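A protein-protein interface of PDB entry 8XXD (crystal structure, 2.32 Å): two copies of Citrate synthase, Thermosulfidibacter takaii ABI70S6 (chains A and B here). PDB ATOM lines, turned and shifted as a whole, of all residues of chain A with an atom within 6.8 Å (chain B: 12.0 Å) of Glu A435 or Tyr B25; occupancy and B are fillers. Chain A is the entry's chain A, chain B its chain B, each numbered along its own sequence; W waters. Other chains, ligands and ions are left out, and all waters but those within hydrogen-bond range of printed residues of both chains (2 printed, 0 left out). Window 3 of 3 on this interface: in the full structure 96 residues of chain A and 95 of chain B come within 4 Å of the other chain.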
ATOM      1  N   THR A  34       6.060   7.222 -20.711  1.00  0.00           N
ATOM      2  CA  THR A  34       6.615   6.073 -21.411  1.00  0.00           C
ATOM      3  C   THR A  34       5.673   4.872 -21.333  1.00  0.00           C
ATOM      4  O   THR A  34       4.703   4.879 -20.560  1.00  0.00           O
ATOM      5  CB  THR A  34       7.968   5.682 -20.801  1.00  0.00           C
ATOM      6  OG1 THR A  34       7.730   5.141 -19.495  1.00  0.00           O
ATOM      7  CG2 THR A  34       8.939   6.851 -20.740  1.00  0.00           C
ATOM      8  N   ILE A  35       6.006   3.839 -22.131  1.00  0.00           N
ATOM      9  CA  ILE A  35       5.341   2.547 -22.129  1.00  0.00           C
ATOM     10  C   ILE A  35       5.460   1.879 -20.763  1.00  0.00           C
ATOM     11  O   ILE A  35       4.559   1.134 -20.353  1.00  0.00           O
ATOM     12  CB  ILE A  35       5.914   1.655 -23.239  1.00  0.00           C
ATOM     13  CG1 ILE A  35       5.494   2.172 -24.614  1.00  0.00           C
ATOM     14  CG2 ILE A  35       5.498   0.204 -23.045  1.00  0.00           C
ATOM     15  CD1 ILE A  35       6.003   1.330 -25.745  1.00  0.00           C
ATOM     16  N   GLY A  36       6.604   2.135 -20.109  1.00  0.00           N
ATOM     17  CA  GLY A  36       6.927   1.632 -18.783  1.00  0.00           C
ATOM     18  C   GLY A  36       5.914   2.078 -17.742  1.00  0.00           C
ATOM     19  O   GLY A  36       5.435   1.228 -16.991  1.00  0.00           O
ATOM     20  N   VAL A 430       1.225  -1.376 -28.725  1.00  0.00           N
ATOM     21  CA  VAL A 430       2.588  -1.429 -28.236  1.00  0.00           C
ATOM     22  C   VAL A 430       3.437  -2.339 -29.129  1.00  0.00           C
ATOM     23  O   VAL A 430       4.511  -1.928 -29.524  1.00  0.00           O
ATOM     24  CB  VAL A 430       2.633  -1.872 -26.758  1.00  0.00           C
ATOM     25  CG1 VAL A 430       4.017  -2.313 -26.319  1.00  0.00           C
ATOM     26  CG2 VAL A 430       2.116  -0.793 -25.829  1.00  0.00           C
ATOM     27  N   LYS A 431       2.987  -3.563 -29.449  1.00  0.00           N
ATOM     28  CA  LYS A 431       3.774  -4.455 -30.303  1.00  0.00           C
ATOM     29  C   LYS A 431       3.913  -3.920 -31.733  1.00  0.00           C
ATOM     30  O   LYS A 431       4.798  -4.346 -32.475  1.00  0.00           O
ATOM     31  CB  LYS A 431       3.146  -5.846 -30.446  1.00  0.00           C
ATOM     32  CG  LYS A 431       3.449  -6.831 -29.324  1.00  0.00           C
ATOM     33  CD  LYS A 431       3.006  -8.236 -29.657  1.00  0.00           C
ATOM     34  CE  LYS A 431       2.440  -8.942 -28.449  1.00  0.00           C
ATOM     35  NZ  LYS A 431       1.653 -10.145 -28.814  1.00  0.00           N
ATOM     36  N   GLU A 432       2.975  -3.064 -32.153  1.00  0.00           N
ATOM     37  CA  GLU A 432       2.961  -2.574 -33.517  1.00  0.00           C
ATOM     38  C   GLU A 432       3.983  -1.446 -33.665  1.00  0.00           C
ATOM     39  O   GLU A 432       4.587  -1.334 -34.715  1.00  0.00           O
ATOM     40  CB  GLU A 432       1.553  -2.108 -33.898  1.00  0.00           C
ATOM     41  CG  GLU A 432       1.343  -1.807 -35.380  1.00  0.00           C
ATOM     42  CD  GLU A 432      -0.018  -1.189 -35.719  1.00  0.00           C
ATOM     43  OE1 GLU A 432      -0.813  -1.841 -36.460  1.00  0.00           O
ATOM     44  OE2 GLU A 432      -0.301  -0.055 -35.243  1.00  0.00           O
ATOM     45  N   VAL A 433       4.127  -0.589 -32.648  1.00  0.00           N
ATOM     46  CA  VAL A 433       4.734   0.712 -32.852  1.00  0.00           C
ATOM     47  C   VAL A 433       5.992   0.876 -32.002  1.00  0.00           C
ATOM     48  O   VAL A 433       6.683   1.870 -32.122  1.00  0.00           O
ATOM     49  CB  VAL A 433       3.725   1.843 -32.570  1.00  0.00           C
ATOM     50  CG1 VAL A 433       2.427   1.671 -33.336  1.00  0.00           C
ATOM     51  CG2 VAL A 433       3.435   1.998 -31.088  1.00  0.00           C
ATOM     52  N   ALA A 434       6.285  -0.065 -31.114  1.00  0.00           N
ATOM     53  CA  ALA A 434       7.283   0.185 -30.086  1.00  0.00           C
ATOM     54  C   ALA A 434       8.651   0.499 -30.705  1.00  0.00           C
ATOM     55  O   ALA A 434       9.262   1.504 -30.331  1.00  0.00           O
ATOM     56  CB  ALA A 434       7.355  -0.976 -29.139  1.00  0.00           C
ATOM     57  N   GLU A 435       9.115  -0.361 -31.625  1.00  0.00           N
ATOM     58  CA  GLU A 435      10.377  -0.162 -32.340  1.00  0.00           C
ATOM     59  C   GLU A 435      10.462   1.239 -32.944  1.00  0.00           C
ATOM     60  O   GLU A 435      11.489   1.874 -32.808  1.00  0.00           O
ATOM     61  CB  GLU A 435      10.596  -1.242 -33.401  1.00  0.00           C
ATOM     62  CG  GLU A 435      11.125  -2.540 -32.822  1.00  0.00           C
ATOM     63  CD  GLU A 435      10.722  -3.811 -33.560  1.00  0.00           C
ATOM     64  OE1 GLU A 435      11.622  -4.655 -33.818  1.00  0.00           O
ATOM     65  OE2 GLU A 435       9.497  -3.983 -33.858  1.00  0.00           O
ATOM     66  N   SER A 436       9.370   1.762 -33.512  1.00  0.00           N
ATOM     67  CA  SER A 436       9.378   3.065 -34.171  1.00  0.00           C
ATOM     68  C   SER A 436       9.381   4.258 -33.195  1.00  0.00           C
ATOM     69  O   SER A 436       9.472   5.414 -33.629  1.00  0.00           O
ATOM     70  CB  SER A 436       8.199   3.158 -35.126  1.00  0.00           C
ATOM     71  OG  SER A 436       7.030   3.617 -34.443  1.00  0.00           O
ATOM     72  N   LEU A 437       9.248   4.007 -31.882  1.00  0.00           N
ATOM     73  CA  LEU A 437       9.142   5.079 -30.902  1.00  0.00           C
ATOM     74  C   LEU A 437      10.527   5.485 -30.409  1.00  0.00           C
ATOM     75  O   LEU A 437      11.427   4.665 -30.200  1.00  0.00           O
ATOM     76  CB  LEU A 437       8.296   4.659 -29.689  1.00  0.00           C
ATOM     77  CG  LEU A 437       6.781   4.542 -29.872  1.00  0.00           C
ATOM     78  CD1 LEU A 437       6.152   4.004 -28.591  1.00  0.00           C
ATOM     79  CD2 LEU A 437       6.146   5.874 -30.252  1.00  0.00           C
ATOM     80  N   PRO A 438      10.684   6.775 -30.082  1.00  0.00           N
ATOM     81  CA  PRO A 438      11.931   7.258 -29.508  1.00  0.00           C
ATOM     82  C   PRO A 438      12.112   6.831 -28.053  1.00  0.00           C
ATOM     83  O   PRO A 438      11.175   6.869 -27.260  1.00  0.00           O
ATOM     84  CB  PRO A 438      11.784   8.790 -29.609  1.00  0.00           C
ATOM     85  CG  PRO A 438      10.279   9.063 -29.595  1.00  0.00           C
ATOM     86  CD  PRO A 438       9.652   7.822 -30.199  1.00  0.00           C
ATOM     87  N   TRP B  14       1.136 -14.787 -22.075  1.00  0.00           N
ATOM     88  CA  TRP B  14       0.943 -13.351 -21.999  1.00  0.00           C
ATOM     89  C   TRP B  14       1.816 -12.797 -20.878  1.00  0.00           C
ATOM     90  O   TRP B  14       2.510 -11.812 -21.052  1.00  0.00           O
ATOM     91  CB  TRP B  14      -0.527 -13.003 -21.792  1.00  0.00           C
ATOM     92  CG  TRP B  14      -1.411 -13.255 -22.973  1.00  0.00           C
ATOM     93  CD1 TRP B  14      -1.056 -13.272 -24.288  1.00  0.00           C
ATOM     94  CD2 TRP B  14      -2.823 -13.521 -22.941  1.00  0.00           C
ATOM     95  NE1 TRP B  14      -2.149 -13.518 -25.074  1.00  0.00           N
ATOM     96  CE2 TRP B  14      -3.246 -13.684 -24.281  1.00  0.00           C
ATOM     97  CE3 TRP B  14      -3.765 -13.649 -21.912  1.00  0.00           C
ATOM     98  CZ2 TRP B  14      -4.567 -13.952 -24.624  1.00  0.00           C
ATOM     99  CZ3 TRP B  14      -5.076 -13.920 -22.252  1.00  0.00           C
ATOM    100  CH2 TRP B  14      -5.465 -14.079 -23.588  1.00  0.00           C
ATOM    101  N   ALA B  16       4.566 -13.807 -19.871  1.00  0.00           N
ATOM    102  CA  ALA B  16       5.967 -13.760 -20.292  1.00  0.00           C
ATOM    103  C   ALA B  16       6.150 -12.662 -21.337  1.00  0.00           C
ATOM    104  O   ALA B  16       7.155 -11.960 -21.298  1.00  0.00           O
ATOM    105  CB  ALA B  16       6.487 -15.100 -20.792  1.00  0.00           C
ATOM    106  N   GLU B  17       5.170 -12.478 -22.231  1.00  0.00           N
ATOM    107  CA  GLU B  17       5.283 -11.430 -23.226  1.00  0.00           C
ATOM    108  C   GLU B  17       5.362 -10.061 -22.543  1.00  0.00           C
ATOM    109  O   GLU B  17       6.186  -9.227 -22.914  1.00  0.00           O
ATOM    110  CB  GLU B  17       4.134 -11.466 -24.235  1.00  0.00           C
ATOM    111  CG  GLU B  17       4.184 -10.324 -25.254  1.00  0.00           C
ATOM    112  CD  GLU B  17       5.399 -10.282 -26.188  1.00  0.00           C
ATOM    113  OE1 GLU B  17       5.811 -11.352 -26.695  1.00  0.00           O
ATOM    114  OE2 GLU B  17       5.938  -9.176 -26.428  1.00  0.00           O
ATOM    115  N   VAL B  18       4.498  -9.831 -21.546  1.00  0.00           N
ATOM    116  CA  VAL B  18       4.453  -8.548 -20.873  1.00  0.00           C
ATOM    117  C   VAL B  18       5.778  -8.303 -20.149  1.00  0.00           C
ATOM    118  O   VAL B  18       6.267  -7.184 -20.151  1.00  0.00           O
ATOM    119  CB  VAL B  18       3.234  -8.441 -19.933  1.00  0.00           C
ATOM    120  CG1 VAL B  18       3.372  -7.306 -18.937  1.00  0.00           C
ATOM    121  CG2 VAL B  18       1.950  -8.310 -20.726  1.00  0.00           C
ATOM    122  N   ALA B  19       6.357  -9.328 -19.513  1.00  0.00           N
ATOM    123  CA  ALA B  19       7.598  -9.120 -18.783  1.00  0.00           C
ATOM    124  C   ALA B  19       8.684  -8.614 -19.754  1.00  0.00           C
ATOM    125  O   ALA B  19       9.437  -7.706 -19.419  1.00  0.00           O
ATOM    126  CB  ALA B  19       7.993 -10.382 -18.046  1.00  0.00           C
ATOM    127  N   GLU B  20       8.706  -9.158 -20.977  1.00  0.00           N
ATOM    128  CA  GLU B  20       9.670  -8.795 -22.005  1.00  0.00           C
ATOM    129  C   GLU B  20       9.425  -7.384 -22.528  1.00  0.00           C
ATOM    130  O   GLU B  20      10.337  -6.567 -22.593  1.00  0.00           O
ATOM    131  CB  GLU B  20       9.568  -9.755 -23.177  1.00  0.00           C
ATOM    132  CG  GLU B  20      10.044 -11.146 -22.827  1.00  0.00           C
ATOM    133  CD  GLU B  20      10.236 -12.019 -24.055  1.00  0.00           C
ATOM    134  OE1 GLU B  20       9.839 -11.566 -25.168  1.00  0.00           O
ATOM    135  OE2 GLU B  20      10.809 -13.125 -23.904  1.00  0.00           O
ATOM    136  N   ILE B  21       8.184  -7.097 -22.910  1.00  0.00           N
ATOM    137  CA  ILE B  21       7.842  -5.756 -23.354  1.00  0.00           C
ATOM    138  C   ILE B  21       8.319  -4.688 -22.370  1.00  0.00           C
ATOM    139  O   ILE B  21       8.788  -3.635 -22.779  1.00  0.00           O
ATOM    140  CB  ILE B  21       6.327  -5.655 -23.575  1.00  0.00           C
ATOM    141  CG1 ILE B  21       5.921  -6.426 -24.827  1.00  0.00           C
ATOM    142  CG2 ILE B  21       5.907  -4.194 -23.610  1.00  0.00           C
ATOM    143  CD1 ILE B  21       4.427  -6.548 -25.017  1.00  0.00           C
ATOM    144  N   ARG B  22       8.094  -4.931 -21.078  1.00  0.00           N
ATOM    145  CA  ARG B  22       8.360  -3.974 -20.024  1.00  0.00           C
ATOM    146  C   ARG B  22       9.872  -3.756 -19.940  1.00  0.00           C
ATOM    147  O   ARG B  22      10.371  -2.690 -19.593  1.00  0.00           O
ATOM    148  CB  ARG B  22       7.804  -4.511 -18.687  1.00  0.00           C
ATOM    149  CG  ARG B  22       6.286  -4.438 -18.518  1.00  0.00           C
ATOM    150  CD  ARG B  22       5.770  -4.816 -17.124  1.00  0.00           C
ATOM    151  NE  ARG B  22       6.243  -3.891 -16.105  1.00  0.00           N
ATOM    152  CZ  ARG B  22       6.311  -4.147 -14.800  1.00  0.00           C
ATOM    153  NH1 ARG B  22       5.947  -5.326 -14.338  1.00  0.00           N
ATOM    154  NH2 ARG B  22       6.730  -3.213 -13.958  1.00  0.00           N
ATOM    155  N   LYS B  23      10.587  -4.839 -20.199  1.00  0.00           N
ATOM    156  CA  LYS B  23      12.029  -4.869 -20.132  1.00  0.00           C
ATOM    157  C   LYS B  23      12.564  -4.138 -21.361  1.00  0.00           C
ATOM    158  O   LYS B  23      13.326  -3.180 -21.225  1.00  0.00           O
ATOM    159  CB  LYS B  23      12.461  -6.334 -20.029  1.00  0.00           C
ATOM    160  CG  LYS B  23      13.876  -6.553 -19.542  1.00  0.00           C
ATOM    161  CD  LYS B  23      14.117  -6.111 -18.128  1.00  0.00           C
ATOM    162  CE  LYS B  23      15.523  -6.446 -17.684  1.00  0.00           C
ATOM    163  NZ  LYS B  23      15.658  -6.370 -16.216  1.00  0.00           N
ATOM    164  N   LYS B  24      12.063  -4.509 -22.549  1.00  0.00           N
ATOM    165  CA  LYS B  24      12.717  -4.107 -23.780  1.00  0.00           C
ATOM    166  C   LYS B  24      12.150  -2.824 -24.369  1.00  0.00           C
ATOM    167  O   LYS B  24      12.903  -2.150 -25.070  1.00  0.00           O
ATOM    168  CB  LYS B  24      12.768  -5.261 -24.770  1.00  0.00           C
ATOM    169  CG  LYS B  24      11.540  -5.516 -25.618  1.00  0.00           C
ATOM    170  CD  LYS B  24      11.757  -6.769 -26.453  1.00  0.00           C
ATOM    171  CE  LYS B  24      10.663  -7.024 -27.461  1.00  0.00           C
ATOM    172  NZ  LYS B  24      10.816  -8.356 -28.080  1.00  0.00           N
ATOM    173  N   TYR B  25      10.909  -2.437 -24.019  1.00  0.00           N
ATOM    174  CA  TYR B  25      10.282  -1.233 -24.561  1.00  0.00           C
ATOM    175  C   TYR B  25       9.893  -0.220 -23.481  1.00  0.00           C
ATOM    176  O   TYR B  25       9.190   0.743 -23.769  1.00  0.00           O
ATOM    177  CB  TYR B  25       9.010  -1.591 -25.357  1.00  0.00           C
ATOM    178  CG  TYR B  25       9.188  -2.469 -26.578  1.00  0.00           C
ATOM    179  CD1 TYR B  25      10.268  -2.310 -27.453  1.00  0.00           C
ATOM    180  CD2 TYR B  25       8.240  -3.417 -26.913  1.00  0.00           C
ATOM    181  CE1 TYR B  25      10.416  -3.088 -28.593  1.00  0.00           C
ATOM    182  CE2 TYR B  25       8.388  -4.229 -28.034  1.00  0.00           C
ATOM    183  CZ  TYR B  25       9.467  -4.051 -28.887  1.00  0.00           C
ATOM    184  OH  TYR B  25       9.588  -4.828 -30.011  1.00  0.00           O
ATOM    185  N   GLY B  26      10.322  -0.429 -22.237  1.00  0.00           N
ATOM    186  CA  GLY B  26       9.849   0.355 -21.103  1.00  0.00           C
ATOM    187  C   GLY B  26      10.211   1.835 -21.157  1.00  0.00           C
ATOM    188  O   GLY B  26       9.440   2.677 -20.704  1.00  0.00           O
ATOM    189  N   ASN B  27      11.384   2.146 -21.726  1.00  0.00           N
ATOM    190  CA  ASN B  27      11.828   3.525 -21.837  1.00  0.00           C
ATOM    191  C   ASN B  27      11.349   4.162 -23.139  1.00  0.00           C
ATOM    192  O   ASN B  27      11.653   5.324 -23.407  1.00  0.00           O
ATOM    193  CB  ASN B  27      13.340   3.688 -21.586  1.00  0.00           C
ATOM    194  CG  ASN B  27      14.276   2.807 -22.390  1.00  0.00           C
ATOM    195  OD1 ASN B  27      15.489   2.910 -22.226  1.00  0.00           O
ATOM    196  ND2 ASN B  27      13.759   1.966 -23.272  1.00  0.00           N
ATOM    197  N   ARG B  28      10.536   3.459 -23.925  1.00  0.00           N
ATOM    198  CA  ARG B  28      10.013   4.063 -25.139  1.00  0.00           C
ATOM    199  C   ARG B  28       9.010   5.162 -24.810  1.00  0.00           C
ATOM    200  O   ARG B  28       8.068   4.945 -24.051  1.00  0.00           O
ATOM    201  CB  ARG B  28       9.371   3.000 -26.018  1.00  0.00           C
ATOM    202  CG  ARG B  28      10.358   1.947 -26.492  1.00  0.00           C
ATOM    203  CD  ARG B  28      11.439   2.530 -27.390  1.00  0.00           C
ATOM    204  NE  ARG B  28      12.400   1.517 -27.811  1.00  0.00           N
ATOM    205  CZ  ARG B  28      12.798   1.307 -29.066  1.00  0.00           C
ATOM    206  NH1 ARG B  28      13.496   0.213 -29.320  1.00  0.00           N
ATOM    207  NH2 ARG B  28      12.460   2.143 -30.052  1.00  0.00           N
ATOM    208  N   LYS B  29       9.206   6.337 -25.410  1.00  0.00           N
ATOM    209  CA  LYS B  29       8.368   7.497 -25.147  1.00  0.00           C
ATOM    210  C   LYS B  29       7.128   7.471 -26.041  1.00  0.00           C
ATOM    211  O   LYS B  29       7.226   7.294 -27.250  1.00  0.00           O
ATOM    212  CB  LYS B  29       9.144   8.813 -25.338  1.00  0.00           C
ATOM    213  CG  LYS B  29       8.277  10.064 -25.381  1.00  0.00           C
ATOM    214  CD  LYS B  29       9.006  11.331 -25.752  1.00  0.00           C
ATOM    215  CE  LYS B  29       8.045  12.486 -25.944  1.00  0.00           C
ATOM    216  NZ  LYS B  29       8.744  13.782 -26.086  1.00  0.00           N
ATOM    217  N   THR B  30       5.972   7.743 -25.423  1.00  0.00           N
ATOM    218  CA  THR B  30       4.680   7.756 -26.095  1.00  0.00           C
ATOM    219  C   THR B  30       4.174   9.190 -26.206  1.00  0.00           C
ATOM    220  O   THR B  30       3.463   9.511 -27.154  1.00  0.00           O
ATOM    221  CB  THR B  30       3.652   6.858 -25.368  1.00  0.00           C
ATOM    222  OG1 THR B  30       3.594   7.236 -23.993  1.00  0.00           O
ATOM    223  CG2 THR B  30       3.991   5.390 -25.426  1.00  0.00           C
ATOM    224  N   MET B  31       4.513  10.048 -25.228  1.00  0.00           N
ATOM    225  CA  MET B  31       4.060  11.425 -25.259  1.00  0.00           C
ATOM    226  C   MET B  31       4.713  12.224 -24.141  1.00  0.00           C
ATOM    227  O   MET B  31       5.413  11.666 -23.287  1.00  0.00           O
ATOM    228  CB  MET B  31       2.538  11.539 -25.113  1.00  0.00           C
ATOM    229  CG  MET B  31       2.002  10.875 -23.864  1.00  0.00           C
ATOM    230  SD  MET B  31       0.170  10.716 -23.868  1.00  0.00           S
ATOM    231  CE  MET B  31      -0.328  12.429 -23.765  1.00  0.00           C
ATOM    232  N   LYS B  46      -1.291   8.512 -21.648  1.00  0.00           N
ATOM    233  CA  LYS B  46      -1.374   7.091 -21.894  1.00  0.00           C
ATOM    234  C   LYS B  46      -0.772   6.372 -20.693  1.00  0.00           C
ATOM    235  O   LYS B  46       0.340   5.860 -20.760  1.00  0.00           O
ATOM    236  CB  LYS B  46      -0.677   6.766 -23.215  1.00  0.00           C
ATOM    237  CG  LYS B  46      -1.324   7.370 -24.453  1.00  0.00           C
ATOM    238  CD  LYS B  46      -0.639   6.934 -25.739  1.00  0.00           C
ATOM    239  CE  LYS B  46      -0.611   8.006 -26.808  1.00  0.00           C
ATOM    240  NZ  LYS B  46      -1.573   7.747 -27.895  1.00  0.00           N
ATOM    241  N   VAL B  49      -2.989   0.231 -19.095  1.00  0.00           N
ATOM    242  CA  VAL B  49      -3.071  -0.895 -20.016  1.00  0.00           C
ATOM    243  C   VAL B  49      -4.463  -1.519 -19.946  1.00  0.00           C
ATOM    244  O   VAL B  49      -4.974  -1.826 -18.879  1.00  0.00           O
ATOM    245  CB  VAL B  49      -2.029  -1.984 -19.696  1.00  0.00           C
ATOM    246  CG1 VAL B  49      -2.154  -3.178 -20.624  1.00  0.00           C
ATOM    247  CG2 VAL B  49      -0.604  -1.461 -19.737  1.00  0.00           C
HETATM  248  O   HOH W   1       2.678   5.309 -22.107  1.00  0.00           O
HETATM  249  O   HOH W   2       2.499 -12.095 -26.720  1.00  0.00           O
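No position is printed for both chains.
The side-chain hydroxyl (OG1) of Thr A34 sits close to the backbone NH (N) of Gly A36, at 3.3 Å.
Of chain B, only Gly B26 (3.2 Å) and Arg B28 (3.2 Å) come within 4 Å of Thr A34. Gly A36 touches just one residue of chain B: Gly B26. No residue of chain B comes within 4 Å of Val A433. Ala A434 touches just these residues of chain B: Tyr B25 and Arg B28. No residue of chain B comes within 4 Å of Ser A436. Leu A437 touches just these residues of chain B: Arg B28 (2.7 Å) and Lys B29 (3.5 Å). Ala B19 touches none of the printed residues of chain A. Of the printed residues of chain A, Ile B21 touches Val A430. Of chain A, only Ile A35 (3.4 Å), Ala A434 (3.4 Å) and Glu A435 (3.9 Å) come within 4 Å of Tyr B25. Of the printed residues of chain A, Arg B28 touches Thr A34 (3.2 Å), Ile A35 (3.0 Å), Ala A434 (3.3 Å), Glu A435 (2.9 Å), Leu A437 (2.7 Å) and Pro A438 (3.7 Å). Lys B46 touches none of the printed residues of chain A. The nearest residue of chain B that does not touch Glu A435 is Lys B24 (6.9 Å). The nearest residue of chain A that does not touch Tyr B25 is Val A430 (4.4 Å). The nearest printed residue of chain B that does not touch Lys A431 is Ile B21 (4.4 Å).
Among the printed residues, merely in contact across the chains: Thr A34 with Arg B28, Ala A434 with Tyr B25, Ile A35 with Tyr B25, Leu A437 with Lys B29, Ile A35 with Thr B30, Pro A438 with Arg B28, Val A430 with Ile B21, Glu A435 with Tyr B25, Lys A431 with Glu B17 and Ile A35 with Gly B26.
The backbone carbonyl oxygen (O) of Glu A435 is in hydrogen-bond range of the guanidinium group (NH2) of Arg B28. O of Gly B26 is in hydrogen-bond range of N of Gly A36 (2.9 Å). O of Gly B26 lies within hydrogen-bond range of OG1 of Thr A34 (3.2 Å). The backbone carbonyl oxygen (O) of Arg B28 sits at hydrogen-bond distance from the backbone NH (N) of Ile A35, 3.0 Å away. The backbone carbonyl oxygen of Ala A434 is in hydrogen-bond range of the guanidinium group of Arg B28 (3.3 Å). The backbone carbonyl oxygen (O) of Pro A438 is in hydrogen-bond range of the backbone NH (N) of Lys B29 (2.8 Å). O of Leu A437 lies within hydrogen-bond range of NH2 of Arg B28.
Water W1 lies within hydrogen-bond range of the backbone carbonyl oxygen of Thr A34, the backbone carbonyl oxygen of Lys B46 and the side-chain hydroxyl of Thr B30. Water W2 bridges the side-chain amino group (NZ) of Lys A431 (3.0 Å) and the side-chain carboxylate (OE1) of Glu B17 (3.4 Å).
Of the 12 printed residues of chain A, 9 touch a printed residue of chain B. Printed residues of chain A that touch a printed residue of chain B: Thr A34, Ile A35, Gly A36, Val A430, Lys A431, Ala A434, Glu A435, Leu A437 and Pro A438. Hydrophobic or aromatic side chains of chain A within 4 Å of the printed part of chain B: Ile A35, Val A430, Ala A434, Leu A437 and Pro A438. Along chain B the printed residues that touch a printed residue of chain A span positions 17 to 30. Among the printed residues, 17 pairs touch across the chains. Among the printed residues, no Asp or Glu carboxylate lies within 4 Å of a Lys or Arg side-chain nitrogen of the other chain.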
